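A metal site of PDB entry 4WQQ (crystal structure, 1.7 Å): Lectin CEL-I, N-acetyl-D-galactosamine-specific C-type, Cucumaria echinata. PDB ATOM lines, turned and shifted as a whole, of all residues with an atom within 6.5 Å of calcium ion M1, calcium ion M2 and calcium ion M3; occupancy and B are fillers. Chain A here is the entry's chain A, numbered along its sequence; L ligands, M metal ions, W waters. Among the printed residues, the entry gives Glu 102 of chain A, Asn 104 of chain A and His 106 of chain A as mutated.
NH2 of Arg 116 lies within hydrogen-bond range of O1 of the ligand, 3.1 Å away.
Of the 20 residues printed, 2 come within 4 Å of calcium ion M3.
Water W2 is bound to calcium ion M1 (2.3 Å).
Calcium ion M1 is bound by O of Glu 110 (2.4 Å).
The side-chain carboxylate (OD1) of Asp 111 binds calcium ion M1 (2.4 Å).
Calcium ion M1 is bound by the side-chain carboxylate (OD2) of Asp 78 (2.5 Å).
Calcium ion M1 is bound by OE2 of Glu 82 (2.5 Å).
The side-chain carboxylate (OD1) of Asp 78 binds calcium ion M1, 2.5 Å away.
OE1 of Glu 82 binds calcium ion M1.
Calcium ion M1 is bound by OD1 of Asn 105 (2.6 Å).
Water W3 bridges O of Asn 108 and ND2 of Asn 105.
Calcium ion M3 is bound by water W1 (2.3 Å), the side-chain carboxylate (OD1) of Asp 111 (2.4 Å), the side-chain carboxylate (OE2) of Glu 82 (2.4 Å), water W3 (2.5 Å) and the side-chain carboxylate (OD2) of Asp 111 (2.5 Å).
The side-chain carboxylate of Asp 125 is in hydrogen-bond range of the backbone NH of Asn 105.
OE2 of Glu 102 lies within salt-bridge range of NH1 of Arg 116.
The side-chain carboxylate of Glu 110 sits close to the side-chain amide oxygen of Asn 126 (3.4 Å).
OE1 of Glu 110 lies close to N of His 106 (3.0 Å).
The side-chain carboxylate (OD2) of Asp 78 lies close to the backbone NH (N) of Gly 83 (2.7 Å).
The side-chain amide oxygen of Asn 104 lies close to the backbone NH of His 106, 3.4 Å away.
The backbone carbonyl oxygen of Asn 126 is in hydrogen-bond range of the backbone NH of Asp 111 (3.1 Å).
Calcium ion M2 is bound by OD1 of Asp 125, at 2.3 Å.
Calcium ion M2 is bound by the side-chain amide oxygen (OD1) of Asn 124, at 2.4 Å.
Calcium ion M2 is bound by OD1 of Asn 104.
Calcium ion M2 is bound by OE1 of Glu 110.
O of Asp 125 binds calcium ion M2 (2.5 Å).
Calcium ion M2 is bound by O3 of the ligand (2.5 Å).
The side-chain carboxylate (OE1) of Glu 102 is bound to calcium ion M2.
Calcium ion M2 is bound by O4 of the ligand.
Along chain A the residues within 4 Å of calcium ion M1 span positions 78 to 111.
The nearest printed residue that does not touch calcium ion M1 is Phe 85 (4.3 Å).
The nearest printed residue that does not touch calcium ion M2 is Asn 126 (4.7 Å).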
ATOM      1  N   ASP A  78       4.598  -3.095  17.818  1.00  0.00           N
ATOM      2  CA  ASP A  78       5.293  -2.950  19.102  1.00  0.00           C
ATOM      3  C   ASP A  78       4.347  -2.897  20.315  1.00  0.00           C
ATOM      4  O   ASP A  78       4.584  -2.179  21.287  1.00  0.00           O
ATOM      5  CB  ASP A  78       6.214  -1.726  19.068  1.00  0.00           C
ATOM      6  CG  ASP A  78       5.461  -0.375  19.158  1.00  0.00           C
ATOM      7  OD1 ASP A  78       4.327  -0.241  18.716  1.00  0.00           O
ATOM      8  OD2 ASP A  78       6.027   0.597  19.647  1.00  0.00           O
ATOM      9  N   LYS A  79       3.258  -3.648  20.208  1.00  0.00           N
ATOM     10  CA  LYS A  79       2.312  -3.862  21.272  1.00  0.00           C
ATOM     11  C   LYS A  79       2.979  -4.344  22.563  1.00  0.00           C
ATOM     12  O   LYS A  79       2.656  -3.858  23.616  1.00  0.00           O
ATOM     13  CB  LYS A  79       1.246  -4.897  20.868  1.00  0.00           C
ATOM     14  CG  LYS A  79       0.240  -5.151  21.945  1.00  0.00           C
ATOM     15  CD  LYS A  79      -0.873  -6.137  21.580  1.00  0.00           C
ATOM     16  CE  LYS A  79      -1.561  -6.528  22.901  1.00  0.00           C
ATOM     17  NZ  LYS A  79      -2.932  -6.994  22.644  1.00  0.00           N
ATOM     18  N   GLU A  82       6.862  -1.468  23.595  1.00  0.00           N
ATOM     19  CA  GLU A  82       6.830  -0.175  22.938  1.00  0.00           C
ATOM     20  C   GLU A  82       8.185   0.292  22.476  1.00  0.00           C
ATOM     21  O   GLU A  82       9.138   0.387  23.275  1.00  0.00           O
ATOM     22  CB  GLU A  82       6.173   0.877  23.842  1.00  0.00           C
ATOM     23  CG  GLU A  82       6.112   2.326  23.329  1.00  0.00           C
ATOM     24  CD  GLU A  82       5.313   2.464  22.048  1.00  0.00           C
ATOM     25  OE1 GLU A  82       5.810   3.184  21.142  1.00  0.00           O
ATOM     26  OE2 GLU A  82       4.258   1.807  21.962  1.00  0.00           O
ATOM     27  N   GLY A  83       8.274   0.668  21.201  1.00  0.00           N
ATOM     28  CA  GLY A  83       9.531   1.150  20.621  1.00  0.00           C
ATOM     29  C   GLY A  83      10.392   0.031  20.094  1.00  0.00           C
ATOM     30  O   GLY A  83      11.329   0.311  19.323  1.00  0.00           O
ATOM     31  N   PHE A  85       9.929  -2.875  17.761  1.00  0.00           N
ATOM     32  CA  PHE A  85       9.045  -3.549  16.811  1.00  0.00           C
ATOM     33  C   PHE A  85       9.509  -4.958  16.559  1.00  0.00           C
ATOM     34  O   PHE A  85      10.706  -5.202  16.514  1.00  0.00           O
ATOM     35  CB  PHE A  85       8.936  -2.737  15.512  1.00  0.00           C
ATOM     36  CG  PHE A  85       7.999  -1.529  15.649  1.00  0.00           C
ATOM     37  CD1 PHE A  85       8.447  -0.344  16.166  1.00  0.00           C
ATOM     38  CD2 PHE A  85       6.641  -1.614  15.325  1.00  0.00           C
ATOM     39  CE1 PHE A  85       7.588   0.741  16.330  1.00  0.00           C
ATOM     40  CE2 PHE A  85       5.789  -0.558  15.474  1.00  0.00           C
ATOM     41  CZ  PHE A  85       6.265   0.635  16.024  1.00  0.00           C
ATOM     42  N   GLY A 101      10.847  10.767  10.358  1.00  0.00           N
ATOM     43  CA  GLY A 101      10.169  10.943  11.647  1.00  0.00           C
ATOM     44  C   GLY A 101       9.349   9.812  12.229  1.00  0.00           C
ATOM     45  O   GLY A 101       8.777   9.950  13.329  1.00  0.00           O
ATOM     46  N   GLU A 102       9.354   8.659  11.534  1.00  0.00           N
ATOM     47  CA  GLU A 102       8.682   7.470  12.067  1.00  0.00           C
ATOM     48  C   GLU A 102       9.749   6.501  12.641  1.00  0.00           C
ATOM     49  O   GLU A 102      10.919   6.541  12.160  1.00  0.00           O
ATOM     50  CB  GLU A 102       7.924   6.813  10.917  1.00  0.00           C
ATOM     51  CG  GLU A 102       7.005   7.785  10.210  1.00  0.00           C
ATOM     52  CD  GLU A 102       5.842   8.358  11.051  1.00  0.00           C
ATOM     53  OE1 GLU A 102       5.561   7.809  12.128  1.00  0.00           O
ATOM     54  OE2 GLU A 102       5.176   9.367  10.621  1.00  0.00           O
ATOM     55  N   PRO A 103       9.364   5.618  13.570  1.00  0.00           N
ATOM     56  CA  PRO A 103       7.978   5.517  14.146  1.00  0.00           C
ATOM     57  C   PRO A 103       7.803   6.610  15.190  1.00  0.00           C
ATOM     58  O   PRO A 103       8.739   6.906  15.900  1.00  0.00           O
ATOM     59  CB  PRO A 103       7.983   4.148  14.834  1.00  0.00           C
ATOM     60  CG  PRO A 103       9.392   3.873  15.146  1.00  0.00           C
ATOM     61  CD  PRO A 103      10.226   4.557  14.091  1.00  0.00           C
ATOM     62  N   ASN A 104       6.694   7.292  15.222  1.00  0.00           N
ATOM     63  CA  ASN A 104       6.535   8.365  16.174  1.00  0.00           C
ATOM     64  C   ASN A 104       5.536   8.095  17.265  1.00  0.00           C
ATOM     65  O   ASN A 104       5.296   8.966  18.068  1.00  0.00           O
ATOM     66  CB  ASN A 104       6.193   9.642  15.439  1.00  0.00           C
ATOM     67  CG  ASN A 104       4.843   9.623  14.755  1.00  0.00           C
ATOM     68  OD1 ASN A 104       4.187   8.605  14.653  1.00  0.00           O
ATOM     69  ND2 ASN A 104       4.441  10.749  14.245  1.00  0.00           N
ATOM     70  N   ASN A 105       4.908   6.914  17.297  1.00  0.00           N
ATOM     71  CA  ASN A 105       3.956   6.551  18.363  1.00  0.00           C
ATOM     72  C   ASN A 105       2.966   7.691  18.606  1.00  0.00           C
ATOM     73  O   ASN A 105       2.688   8.079  19.746  1.00  0.00           O
ATOM     74  CB  ASN A 105       4.709   6.148  19.645  1.00  0.00           C
ATOM     75  CG  ASN A 105       3.860   5.350  20.574  1.00  0.00           C
ATOM     76  OD1 ASN A 105       3.102   4.405  20.193  1.00  0.00           O
ATOM     77  ND2 ASN A 105       3.948   5.692  21.846  1.00  0.00           N
ATOM     78  N   HIS A 106       2.406   8.204  17.512  1.00  0.00           N
ATOM     79  CA  HIS A 106       1.679   9.472  17.596  1.00  0.00           C
ATOM     80  C   HIS A 106       0.554   9.370  18.607  1.00  0.00           C
ATOM     81  O   HIS A 106      -0.113   8.334  18.767  1.00  0.00           O
ATOM     82  CB  HIS A 106       1.113   9.847  16.234  1.00  0.00           C
ATOM     83  CG  HIS A 106       0.402  11.153  16.228  1.00  0.00           C
ATOM     84  ND1 HIS A 106       1.083  12.339  16.188  1.00  0.00           N
ATOM     85  CD2 HIS A 106      -0.911  11.455  16.212  1.00  0.00           C
ATOM     86  CE1 HIS A 106       0.221  13.341  16.142  1.00  0.00           C
ATOM     87  NE2 HIS A 106      -0.996  12.827  16.192  1.00  0.00           N
ATOM     88  N   ASN A 108       0.755   8.758  21.579  1.00  0.00           N
ATOM     89  CA  ASN A 108       1.032   7.638  22.418  1.00  0.00           C
ATOM     90  C   ASN A 108       0.270   6.366  22.120  1.00  0.00           C
ATOM     91  O   ASN A 108       0.078   5.581  23.029  1.00  0.00           O
ATOM     92  CB  ASN A 108       0.784   7.946  23.915  1.00  0.00           C
ATOM     93  CG  ASN A 108       1.749   8.942  24.442  1.00  0.00           C
ATOM     94  OD1 ASN A 108       2.732   8.595  25.089  1.00  0.00           O
ATOM     95  ND2 ASN A 108       1.494  10.190  24.179  1.00  0.00           N
ATOM     96  N   ALA A 109      -0.136   6.143  20.865  1.00  0.00           N
ATOM     97  CA  ALA A 109      -1.083   5.114  20.503  1.00  0.00           C
ATOM     98  C   ALA A 109      -0.919   4.614  19.091  1.00  0.00           C
ATOM     99  O   ALA A 109      -1.872   4.603  18.337  1.00  0.00           O
ATOM    100  CB  ALA A 109      -2.497   5.648  20.660  1.00  0.00           C
ATOM    101  N   GLU A 110       0.304   4.304  18.698  1.00  0.00           N
ATOM    102  CA  GLU A 110       0.531   3.753  17.384  1.00  0.00           C
ATOM    103  C   GLU A 110       1.477   2.595  17.527  1.00  0.00           C
ATOM    104  O   GLU A 110       2.712   2.765  17.711  1.00  0.00           O
ATOM    105  CB  GLU A 110       1.054   4.803  16.390  1.00  0.00           C
ATOM    106  CG  GLU A 110       0.068   5.918  16.070  1.00  0.00           C
ATOM    107  CD  GLU A 110       0.512   6.753  14.884  1.00  0.00           C
ATOM    108  OE1 GLU A 110       1.745   7.050  14.815  1.00  0.00           O
ATOM    109  OE2 GLU A 110      -0.349   7.154  14.045  1.00  0.00           O
ATOM    110  N   ASP A 111       0.906   1.393  17.372  1.00  0.00           N
ATOM    111  CA  ASP A 111       1.670   0.193  17.537  1.00  0.00           C
ATOM    112  C   ASP A 111       1.798  -0.710  16.280  1.00  0.00           C
ATOM    113  O   ASP A 111       2.282  -1.808  16.366  1.00  0.00           O
ATOM    114  CB  ASP A 111       1.157  -0.610  18.738  1.00  0.00           C
ATOM    115  CG  ASP A 111       1.417   0.085  20.125  1.00  0.00           C
ATOM    116  OD1 ASP A 111       2.103   1.162  20.239  1.00  0.00           O
ATOM    117  OD2 ASP A 111       0.923  -0.497  21.135  1.00  0.00           O
ATOM    118  N   TYR A 112       1.335  -0.261  15.131  1.00  0.00           N
ATOM    119  CA  TYR A 112       1.088  -1.148  13.975  1.00  0.00           C
ATOM    120  C   TYR A 112       1.726  -0.587  12.731  1.00  0.00           C
ATOM    121  O   TYR A 112       1.437   0.544  12.318  1.00  0.00           O
ATOM    122  CB  TYR A 112      -0.438  -1.463  13.804  1.00  0.00           C
ATOM    123  CG  TYR A 112      -0.961  -1.995  15.069  1.00  0.00           C
ATOM    124  CD1 TYR A 112      -0.639  -3.303  15.466  1.00  0.00           C
ATOM    125  CD2 TYR A 112      -1.596  -1.148  15.998  1.00  0.00           C
ATOM    126  CE1 TYR A 112      -1.007  -3.787  16.692  1.00  0.00           C
ATOM    127  CE2 TYR A 112      -1.967  -1.640  17.245  1.00  0.00           C
ATOM    128  CZ  TYR A 112      -1.689  -2.951  17.566  1.00  0.00           C
ATOM    129  OH  TYR A 112      -2.068  -3.414  18.841  1.00  0.00           O
ATOM    130  N   ARG A 116       3.562   3.420   3.547  1.00  0.00           N
ATOM    131  CA  ARG A 116       2.978   4.518   2.773  1.00  0.00           C
ATOM    132  C   ARG A 116       2.968   4.195   1.275  1.00  0.00           C
ATOM    133  O   ARG A 116       3.716   3.351   0.815  1.00  0.00           O
ATOM    134  CB  ARG A 116       3.849   5.788   2.999  1.00  0.00           C
ATOM    135  CG  ARG A 116       3.917   6.074   4.459  1.00  0.00           C
ATOM    136  CD  ARG A 116       4.117   7.495   4.814  1.00  0.00           C
ATOM    137  NE  ARG A 116       2.926   7.905   5.561  1.00  0.00           N
ATOM    138  CZ  ARG A 116       2.925   8.509   6.760  1.00  0.00           C
ATOM    139  NH1 ARG A 116       4.075   8.849   7.445  1.00  0.00           N
ATOM    140  NH2 ARG A 116       1.743   8.785   7.292  1.00  0.00           N
ATOM    141  N   ASN A 124       5.336   3.617   8.219  1.00  0.00           N
ATOM    142  CA  ASN A 124       4.756   4.390   9.280  1.00  0.00           C
ATOM    143  C   ASN A 124       4.151   3.430  10.331  1.00  0.00           C
ATOM    144  O   ASN A 124       3.708   2.323   9.987  1.00  0.00           O
ATOM    145  CB  ASN A 124       3.656   5.221   8.698  1.00  0.00           C
ATOM    146  CG  ASN A 124       2.943   6.033   9.731  1.00  0.00           C
ATOM    147  OD1 ASN A 124       3.540   6.651  10.612  1.00  0.00           O
ATOM    148  ND2 ASN A 124       1.617   5.995   9.661  1.00  0.00           N
ATOM    149  N   ASP A 125       4.162   3.850  11.590  1.00  0.00           N
ATOM    150  CA  ASP A 125       3.366   3.254  12.631  1.00  0.00           C
ATOM    151  C   ASP A 125       1.999   3.948  12.705  1.00  0.00           C
ATOM    152  O   ASP A 125       1.889   5.192  12.615  1.00  0.00           O
ATOM    153  CB  ASP A 125       4.092   3.203  13.984  1.00  0.00           C
ATOM    154  CG  ASP A 125       4.483   4.605  14.523  1.00  0.00           C
ATOM    155  OD1 ASP A 125       4.557   5.619  13.763  1.00  0.00           O
ATOM    156  OD2 ASP A 125       4.777   4.664  15.703  1.00  0.00           O
ATOM    157  N   ASN A 126       0.977   3.141  12.932  1.00  0.00           N
ATOM    158  CA  ASN A 126      -0.353   3.700  13.021  1.00  0.00           C
ATOM    159  C   ASN A 126      -1.131   2.960  14.138  1.00  0.00           C
ATOM    160  O   ASN A 126      -0.629   2.019  14.786  1.00  0.00           O
ATOM    161  CB  ASN A 126      -1.031   3.657  11.642  1.00  0.00           C
ATOM    162  CG  ASN A 126      -1.970   4.848  11.387  1.00  0.00           C
ATOM    163  OD1 ASN A 126      -2.656   5.330  12.299  1.00  0.00           O
ATOM    164  ND2 ASN A 126      -2.028   5.327  10.120  1.00  0.00           N
HETATM  165  C1  LIG L   1       0.460  11.635  10.220  1.00  0.00           C
HETATM  166  C2  LIG L   1       1.792  11.273  10.820  1.00  0.00           C
HETATM  167  C3  LIG L   1       1.947   9.772  11.036  1.00  0.00           C
HETATM  168  C4  LIG L   1       0.691   9.236  11.693  1.00  0.00           C
HETATM  169  C5  LIG L   1      -0.486   9.496  10.716  1.00  0.00           C
HETATM  170  C6  LIG L   1      -1.836   8.960  11.106  1.00  0.00           C
HETATM  171  O1  LIG L   1       0.608  11.257   8.873  1.00  0.00           O
HETATM  172  O2  LIG L   1       1.758  11.902  12.079  1.00  0.00           O
HETATM  173  O3  LIG L   1       3.057   9.593  11.916  1.00  0.00           O
HETATM  174  O4  LIG L   1       0.916   7.859  11.928  1.00  0.00           O
HETATM  175  O5  LIG L   1      -0.677  10.954  10.772  1.00  0.00           O
HETATM  176  O6  LIG L   1      -1.915   9.478  12.414  1.00  0.00           O
HETATM  177 CA    CA M   1       4.145   2.166  19.476  1.00  0.00          CA
HETATM  178 CA    CA M   2       3.211   7.266  12.892  1.00  0.00          CA
HETATM  179 CA    CA M   3       2.041   1.102  22.650  1.00  0.00          CA
HETATM  180  O   HOH W   1       3.260  -0.734  23.252  1.00  0.00           O
HETATM  181  O   HOH W   2       5.489   3.311  17.928  1.00  0.00           O
HETATM  182  O   HOH W   3       1.737   3.519  22.279  1.00  0.00           O
